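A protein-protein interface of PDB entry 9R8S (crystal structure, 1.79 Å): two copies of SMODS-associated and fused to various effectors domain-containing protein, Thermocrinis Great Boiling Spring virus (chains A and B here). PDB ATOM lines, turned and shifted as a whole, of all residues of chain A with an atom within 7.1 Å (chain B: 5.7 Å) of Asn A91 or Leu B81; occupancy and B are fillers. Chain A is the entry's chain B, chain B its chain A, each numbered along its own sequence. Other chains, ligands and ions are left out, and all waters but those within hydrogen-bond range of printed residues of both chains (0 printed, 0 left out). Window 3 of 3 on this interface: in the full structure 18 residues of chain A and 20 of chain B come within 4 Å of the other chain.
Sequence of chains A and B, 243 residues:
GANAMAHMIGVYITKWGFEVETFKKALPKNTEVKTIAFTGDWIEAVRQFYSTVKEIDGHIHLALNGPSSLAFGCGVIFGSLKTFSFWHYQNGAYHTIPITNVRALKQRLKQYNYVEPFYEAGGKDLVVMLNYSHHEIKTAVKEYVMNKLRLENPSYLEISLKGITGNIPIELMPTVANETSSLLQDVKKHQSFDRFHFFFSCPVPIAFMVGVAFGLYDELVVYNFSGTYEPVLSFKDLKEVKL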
ATOM      1  N   TRP A  16      16.860  23.568  -3.773  1.00  0.00           N
ATOM      2  CA  TRP A  16      16.412  24.203  -5.004  1.00  0.00           C
ATOM      3  C   TRP A  16      14.906  23.983  -5.172  1.00  0.00           C
ATOM      4  O   TRP A  16      14.118  24.623  -4.475  1.00  0.00           O
ATOM      5  CB  TRP A  16      17.241  23.699  -6.196  1.00  0.00           C
ATOM      6  CG  TRP A  16      18.723  23.927  -6.048  1.00  0.00           C
ATOM      7  CD1 TRP A  16      19.330  24.936  -5.361  1.00  0.00           C
ATOM      8  CD2 TRP A  16      19.788  23.118  -6.603  1.00  0.00           C
ATOM      9  NE1 TRP A  16      20.692  24.816  -5.446  1.00  0.00           N
ATOM     10  CE2 TRP A  16      21.005  23.714  -6.200  1.00  0.00           C
ATOM     11  CE3 TRP A  16      19.837  21.965  -7.400  1.00  0.00           C
ATOM     12  CZ2 TRP A  16      22.248  23.192  -6.567  1.00  0.00           C
ATOM     13  CZ3 TRP A  16      21.066  21.454  -7.765  1.00  0.00           C
ATOM     14  CH2 TRP A  16      22.253  22.061  -7.354  1.00  0.00           C
ATOM     15  N   ASN A  65      18.210  16.774  -1.104  1.00  0.00           N
ATOM     16  CA  ASN A  65      19.235  17.517  -1.813  1.00  0.00           C
ATOM     17  C   ASN A  65      19.586  18.721  -0.945  1.00  0.00           C
ATOM     18  O   ASN A  65      18.931  19.757  -0.997  1.00  0.00           O
ATOM     19  CB  ASN A  65      18.759  17.916  -3.207  1.00  0.00           C
ATOM     20  CG  ASN A  65      19.825  18.662  -3.976  1.00  0.00           C
ATOM     21  OD1 ASN A  65      21.009  18.565  -3.630  1.00  0.00           O
ATOM     22  ND2 ASN A  65      19.446  19.401  -5.013  1.00  0.00           N
ATOM     23  N   HIS A  88      19.262   7.973  -3.187  1.00  0.00           N
ATOM     24  CA  HIS A  88      20.509   8.715  -3.219  1.00  0.00           C
ATOM     25  C   HIS A  88      20.972   8.874  -4.665  1.00  0.00           C
ATOM     26  O   HIS A  88      20.916   7.921  -5.455  1.00  0.00           O
ATOM     27  CB  HIS A  88      21.567   7.973  -2.399  1.00  0.00           C
ATOM     28  CG  HIS A  88      22.893   8.651  -2.306  1.00  0.00           C
ATOM     29  ND1 HIS A  88      23.110   9.816  -1.602  1.00  0.00           N
ATOM     30  CD2 HIS A  88      24.089   8.282  -2.797  1.00  0.00           C
ATOM     31  CE1 HIS A  88      24.390  10.150  -1.697  1.00  0.00           C
ATOM     32  NE2 HIS A  88      25.010   9.225  -2.416  1.00  0.00           N
ATOM     33  N   TYR A  89      21.429  10.087  -4.987  1.00  0.00           N
ATOM     34  CA  TYR A  89      21.852  10.436  -6.328  1.00  0.00           C
ATOM     35  C   TYR A  89      23.339  10.125  -6.459  1.00  0.00           C
ATOM     36  O   TYR A  89      24.137  10.678  -5.709  1.00  0.00           O
ATOM     37  CB  TYR A  89      21.594  11.916  -6.644  1.00  0.00           C
ATOM     38  CG  TYR A  89      21.790  12.233  -8.121  1.00  0.00           C
ATOM     39  CD1 TYR A  89      20.774  11.997  -9.037  1.00  0.00           C
ATOM     40  CD2 TYR A  89      23.004  12.715  -8.606  1.00  0.00           C
ATOM     41  CE1 TYR A  89      20.950  12.250 -10.387  1.00  0.00           C
ATOM     42  CE2 TYR A  89      23.198  12.957  -9.956  1.00  0.00           C
ATOM     43  CZ  TYR A  89      22.166  12.726 -10.848  1.00  0.00           C
ATOM     44  OH  TYR A  89      22.350  12.965 -12.177  1.00  0.00           O
ATOM     45  N   GLN A  90      23.683   9.244  -7.407  1.00  0.00           N
ATOM     46  CA  GLN A  90      25.064   8.845  -7.623  1.00  0.00           C
ATOM     47  C   GLN A  90      25.296   8.518  -9.092  1.00  0.00           C
ATOM     48  O   GLN A  90      24.393   8.042  -9.778  1.00  0.00           O
ATOM     49  CB  GLN A  90      25.346   7.583  -6.819  1.00  0.00           C
ATOM     50  CG  GLN A  90      24.677   6.334  -7.382  1.00  0.00           C
ATOM     51  CD  GLN A  90      25.013   5.081  -6.603  1.00  0.00           C
ATOM     52  OE1 GLN A  90      25.815   5.097  -5.660  1.00  0.00           O
ATOM     53  NE2 GLN A  90      24.405   3.973  -7.002  1.00  0.00           N
ATOM     54  N   ASN A  91      26.536   8.770  -9.537  1.00  0.00           N
ATOM     55  CA  ASN A  91      27.076   8.289 -10.801  1.00  0.00           C
ATOM     56  C   ASN A  91      25.956   7.958 -11.792  1.00  0.00           C
ATOM     57  O   ASN A  91      25.849   6.819 -12.247  1.00  0.00           O
ATOM     58  CB  ASN A  91      27.994   7.081 -10.596  1.00  0.00           C
ATOM     59  CG  ASN A  91      29.128   7.305  -9.615  1.00  0.00           C
ATOM     60  OD1 ASN A  91      30.067   8.070  -9.881  1.00  0.00           O
ATOM     61  ND2 ASN A  91      29.118   6.579  -8.504  1.00  0.00           N
ATOM     62  N   GLY A  92      25.118   8.954 -12.107  1.00  0.00           N
ATOM     63  CA  GLY A  92      24.103   8.810 -13.142  1.00  0.00           C
ATOM     64  C   GLY A  92      22.706   9.221 -12.676  1.00  0.00           C
ATOM     65  O   GLY A  92      22.065  10.053 -13.312  1.00  0.00           O
ATOM     66  N   ALA A  93      22.198   8.600 -11.602  1.00  0.00           N
ATOM     67  CA  ALA A  93      20.785   8.731 -11.270  1.00  0.00           C
ATOM     68  C   ALA A  93      20.529   8.457  -9.787  1.00  0.00           C
ATOM     69  O   ALA A  93      21.463   8.331  -8.992  1.00  0.00           O
ATOM     70  CB  ALA A  93      19.962   7.819 -12.164  1.00  0.00           C
ATOM     71  N   HIS A  95      19.245   6.052  -6.796  1.00  0.00           N
ATOM     72  CA  HIS A  95      19.206   4.641  -6.473  1.00  0.00           C
ATOM     73  C   HIS A  95      18.728   4.479  -5.034  1.00  0.00           C
ATOM     74  O   HIS A  95      19.096   5.266  -4.165  1.00  0.00           O
ATOM     75  CB  HIS A  95      20.582   4.026  -6.729  1.00  0.00           C
ATOM     76  CG  HIS A  95      20.887   3.901  -8.186  1.00  0.00           C
ATOM     77  ND1 HIS A  95      21.648   4.815  -8.885  1.00  0.00           N
ATOM     78  CD2 HIS A  95      20.542   2.950  -9.068  1.00  0.00           C
ATOM     79  CE1 HIS A  95      21.751   4.425 -10.147  1.00  0.00           C
ATOM     80  NE2 HIS A  95      21.081   3.297 -10.282  1.00  0.00           N
ATOM     81  N   ASN A 167      34.361   6.680   0.059  1.00  0.00           N
ATOM     82  CA  ASN A 167      33.834   5.877  -1.026  1.00  0.00           C
ATOM     83  C   ASN A 167      32.905   4.824  -0.438  1.00  0.00           C
ATOM     84  O   ASN A 167      33.222   3.641  -0.435  1.00  0.00           O
ATOM     85  CB  ASN A 167      34.967   5.275  -1.862  1.00  0.00           C
ATOM     86  CG  ASN A 167      34.464   4.431  -3.013  1.00  0.00           C
ATOM     87  OD1 ASN A 167      33.313   4.565  -3.450  1.00  0.00           O
ATOM     88  ND2 ASN A 167      35.319   3.566  -3.535  1.00  0.00           N
ATOM     89  N   ASP B  57      23.831  15.978 -16.714  1.00  0.00           N
ATOM     90  CA  ASP B  57      23.868  15.002 -15.635  1.00  0.00           C
ATOM     91  C   ASP B  57      24.587  13.729 -16.080  1.00  0.00           C
ATOM     92  O   ASP B  57      25.257  13.092 -15.268  1.00  0.00           O
ATOM     93  CB  ASP B  57      22.469  14.672 -15.135  1.00  0.00           C
ATOM     94  CG  ASP B  57      21.764  15.753 -14.324  1.00  0.00           C
ATOM     95  OD1 ASP B  57      22.337  16.852 -14.164  1.00  0.00           O
ATOM     96  OD2 ASP B  57      20.642  15.485 -13.849  1.00  0.00           O
ATOM     97  N   PHE B  78      33.752  21.443 -11.302  1.00  0.00           N
ATOM     98  CA  PHE B  78      33.028  20.368 -11.961  1.00  0.00           C
ATOM     99  C   PHE B  78      32.104  19.667 -10.966  1.00  0.00           C
ATOM    100  O   PHE B  78      31.028  19.213 -11.332  1.00  0.00           O
ATOM    101  CB  PHE B  78      33.997  19.356 -12.577  1.00  0.00           C
ATOM    102  CG  PHE B  78      33.353  18.287 -13.447  1.00  0.00           C
ATOM    103  CD1 PHE B  78      32.853  18.589 -14.709  1.00  0.00           C
ATOM    104  CD2 PHE B  78      33.301  16.968 -13.020  1.00  0.00           C
ATOM    105  CE1 PHE B  78      32.281  17.607 -15.499  1.00  0.00           C
ATOM    106  CE2 PHE B  78      32.749  15.984 -13.820  1.00  0.00           C
ATOM    107  CZ  PHE B  78      32.243  16.302 -15.059  1.00  0.00           C
ATOM    108  N   GLY B  79      32.534  19.582  -9.703  1.00  0.00           N
ATOM    109  CA  GLY B  79      31.832  18.812  -8.689  1.00  0.00           C
ATOM    110  C   GLY B  79      32.146  17.324  -8.829  1.00  0.00           C
ATOM    111  O   GLY B  79      32.911  16.907  -9.708  1.00  0.00           O
ATOM    112  N   SER B  80      31.519  16.511  -7.977  1.00  0.00           N
ATOM    113  CA  SER B  80      31.813  15.090  -7.936  1.00  0.00           C
ATOM    114  C   SER B  80      30.540  14.242  -7.991  1.00  0.00           C
ATOM    115  O   SER B  80      30.533  13.130  -7.493  1.00  0.00           O
ATOM    116  CB  SER B  80      32.683  14.769  -6.746  1.00  0.00           C
ATOM    117  OG  SER B  80      32.150  15.301  -5.544  1.00  0.00           O
ATOM    118  N   LEU B  81      29.497  14.742  -8.672  1.00  0.00           N
ATOM    119  CA  LEU B  81      28.294  13.966  -8.917  1.00  0.00           C
ATOM    120  C   LEU B  81      28.300  13.371 -10.325  1.00  0.00           C
ATOM    121  O   LEU B  81      27.595  12.403 -10.569  1.00  0.00           O
ATOM    122  CB  LEU B  81      27.045  14.818  -8.701  1.00  0.00           C
ATOM    123  CG  LEU B  81      26.745  15.220  -7.256  1.00  0.00           C
ATOM    124  CD1 LEU B  81      25.431  16.008  -7.224  1.00  0.00           C
ATOM    125  CD2 LEU B  81      26.684  14.008  -6.324  1.00  0.00           C
ATOM    126  N   LYS B  82      29.090  13.935 -11.248  1.00  0.00           N
ATOM    127  CA  LYS B  82      29.014  13.569 -12.655  1.00  0.00           C
ATOM    128  C   LYS B  82      30.184  12.659 -13.029  1.00  0.00           C
ATOM    129  O   LYS B  82      31.311  12.928 -12.621  1.00  0.00           O
ATOM    130  CB  LYS B  82      29.117  14.807 -13.552  1.00  0.00           C
ATOM    131  CG  LYS B  82      27.938  15.768 -13.535  1.00  0.00           C
ATOM    132  CD  LYS B  82      28.079  16.913 -14.532  1.00  0.00           C
ATOM    133  CE  LYS B  82      29.069  17.991 -14.168  1.00  0.00           C
ATOM    134  NZ  LYS B  82      28.437  19.128 -13.484  1.00  0.00           N
ATOM    135  N   THR B  83      29.904  11.613 -13.822  1.00  0.00           N
ATOM    136  CA  THR B  83      30.950  10.738 -14.326  1.00  0.00           C
ATOM    137  C   THR B  83      31.536  11.390 -15.571  1.00  0.00           C
ATOM    138  O   THR B  83      30.903  12.222 -16.209  1.00  0.00           O
ATOM    139  CB  THR B  83      30.414   9.337 -14.630  1.00  0.00           C
ATOM    140  OG1 THR B  83      29.455   9.442 -15.674  1.00  0.00           O
ATOM    141  CG2 THR B  83      29.746   8.677 -13.435  1.00  0.00           C
ATOM    142  N   THR B 100      33.902   6.006 -14.100  1.00  0.00           N
ATOM    143  CA  THR B 100      32.495   5.665 -13.973  1.00  0.00           C
ATOM    144  C   THR B 100      32.074   5.610 -12.504  1.00  0.00           C
ATOM    145  O   THR B 100      30.881   5.559 -12.230  1.00  0.00           O
ATOM    146  CB  THR B 100      32.215   4.338 -14.675  1.00  0.00           C
ATOM    147  OG1 THR B 100      32.989   3.341 -14.017  1.00  0.00           O
ATOM    148  CG2 THR B 100      32.582   4.375 -16.143  1.00  0.00           C
ATOM    149  N   ASN B 101      33.043   5.612 -11.580  1.00  0.00           N
ATOM    150  CA  ASN B 101      32.757   5.839 -10.175  1.00  0.00           C
ATOM    151  C   ASN B 101      33.663   6.952  -9.651  1.00  0.00           C
ATOM    152  O   ASN B 101      34.816   6.709  -9.299  1.00  0.00           O
ATOM    153  CB  ASN B 101      32.901   4.557  -9.374  1.00  0.00           C
ATOM    154  CG  ASN B 101      32.672   4.762  -7.896  1.00  0.00           C
ATOM    155  OD1 ASN B 101      32.202   5.812  -7.440  1.00  0.00           O
ATOM    156  ND2 ASN B 101      33.021   3.758  -7.116  1.00  0.00           N
ATOM    157  N   VAL B 102      33.099   8.162  -9.552  1.00  0.00           N
ATOM    158  CA  VAL B 102      33.844   9.346  -9.142  1.00  0.00           C
ATOM    159  C   VAL B 102      34.351   9.170  -7.704  1.00  0.00           C
ATOM    160  O   VAL B 102      35.426   9.648  -7.370  1.00  0.00           O
ATOM    161  CB  VAL B 102      33.015  10.643  -9.308  1.00  0.00           C
ATOM    162  CG1 VAL B 102      33.747  11.882  -8.791  1.00  0.00           C
ATOM    163  CG2 VAL B 102      32.634  10.893 -10.753  1.00  0.00           C
ATOM    164  N   ARG B 103      33.600   8.446  -6.866  1.00  0.00           N
ATOM    165  CA  ARG B 103      33.976   8.244  -5.475  1.00  0.00           C
ATOM    166  C   ARG B 103      35.285   7.466  -5.364  1.00  0.00           C
ATOM    167  O   ARG B 103      35.991   7.610  -4.359  1.00  0.00           O
ATOM    168  CB  ARG B 103      32.848   7.589  -4.673  1.00  0.00           C
ATOM    169  CG  ARG B 103      31.752   8.586  -4.339  1.00  0.00           C
ATOM    170  CD  ARG B 103      30.592   7.912  -3.627  1.00  0.00           C
ATOM    171  NE  ARG B 103      29.844   7.011  -4.519  1.00  0.00           N
ATOM    172  CZ  ARG B 103      29.878   5.675  -4.538  1.00  0.00           C
ATOM    173  NH1 ARG B 103      30.687   4.999  -3.744  1.00  0.00           N
ATOM    174  NH2 ARG B 103      29.109   5.006  -5.382  1.00  0.00           N
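The side-chain carboxylate (OD2) of Asp B57 sits close to the side-chain hydroxyl (OH) of Tyr A89 (3.5 Å). ND2 of Asn A91 sits at hydrogen-bond distance from OD1 of Asn B101 (3.4 Å). N of Val B102 is in hydrogen-bond range of OD1 of Asn A91 (3.1 Å). NH2 of Arg B103 sits at hydrogen-bond distance from OE1 of Gln A90 (3.3 Å). The guanidinium group (NH2) of Arg B103 sits close to the side-chain amide nitrogen (ND2) of Asn A91. The side-chain amide oxygen (OD1) of Asn A167 is in hydrogen-bond range of the guanidinium group (NH1) of Arg B103, 2.7 Å away.
The side-chain amide oxygen (OD1) of Asn B101 lies within hydrogen-bond range of the backbone NH (N) of Arg B103 (3.0 Å). The side-chain hydroxyl of Tyr A89 is in hydrogen-bond range of the backbone carbonyl oxygen of Gly A92. NE2 of Gln A90 sits at hydrogen-bond distance from ND1 of His A95, at 3.4 Å.
Asn A91 touches Leu B81 (N to O, 3.9 Å). CG2 of Thr B83 touches OD1 of Asn A91 (3.6 Å). O of Thr B100 touches OD1 of Asn A91, 3.5 Å away. OD1 of Asn A167 touches ND2 of Asn B101, at 3.8 Å.
Of chain B, only Leu B81 (3.9 Å), Thr B83 (3.6 Å), Thr B100 (3.5 Å), Asn B101 (3.4 Å), Val B102 (3.1 Å) and Arg B103 (3.5 Å) come within 4 Å of Asn A91. Printed residues of chain B within 4 Å of Asn A167: Asn B101 (3.8 Å) and Arg B103 (2.7 Å). Leu B81 touches just one residue of chain A: Asn A91 (3.9 Å). Of the printed residues of chain A, Thr B100 touches Asn A91 (3.5 Å). Printed residues of chain A within 4 Å of Asn B101: Asn A91 and Asn A167. Of the printed residues of chain A, Val B102 touches Asn A91 (3.1 Å). The nearest residue of chain B that does not touch Asn A91 is Lys B82 (5.6 Å).
Along chain A the printed residues that touch a printed residue of chain B span positions 89 to 167. Among the printed residues, 10 pairs touch across the chains. Among the printed residues, no Asp or Glu carboxylate lies within 4 Å of a Lys or Arg side-chain nitrogen of the other chain.
No position is printed for both chains. Of the 10 pairs that touch across the chains among the printed residues, none has its exchanged pair printed and touching as well.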
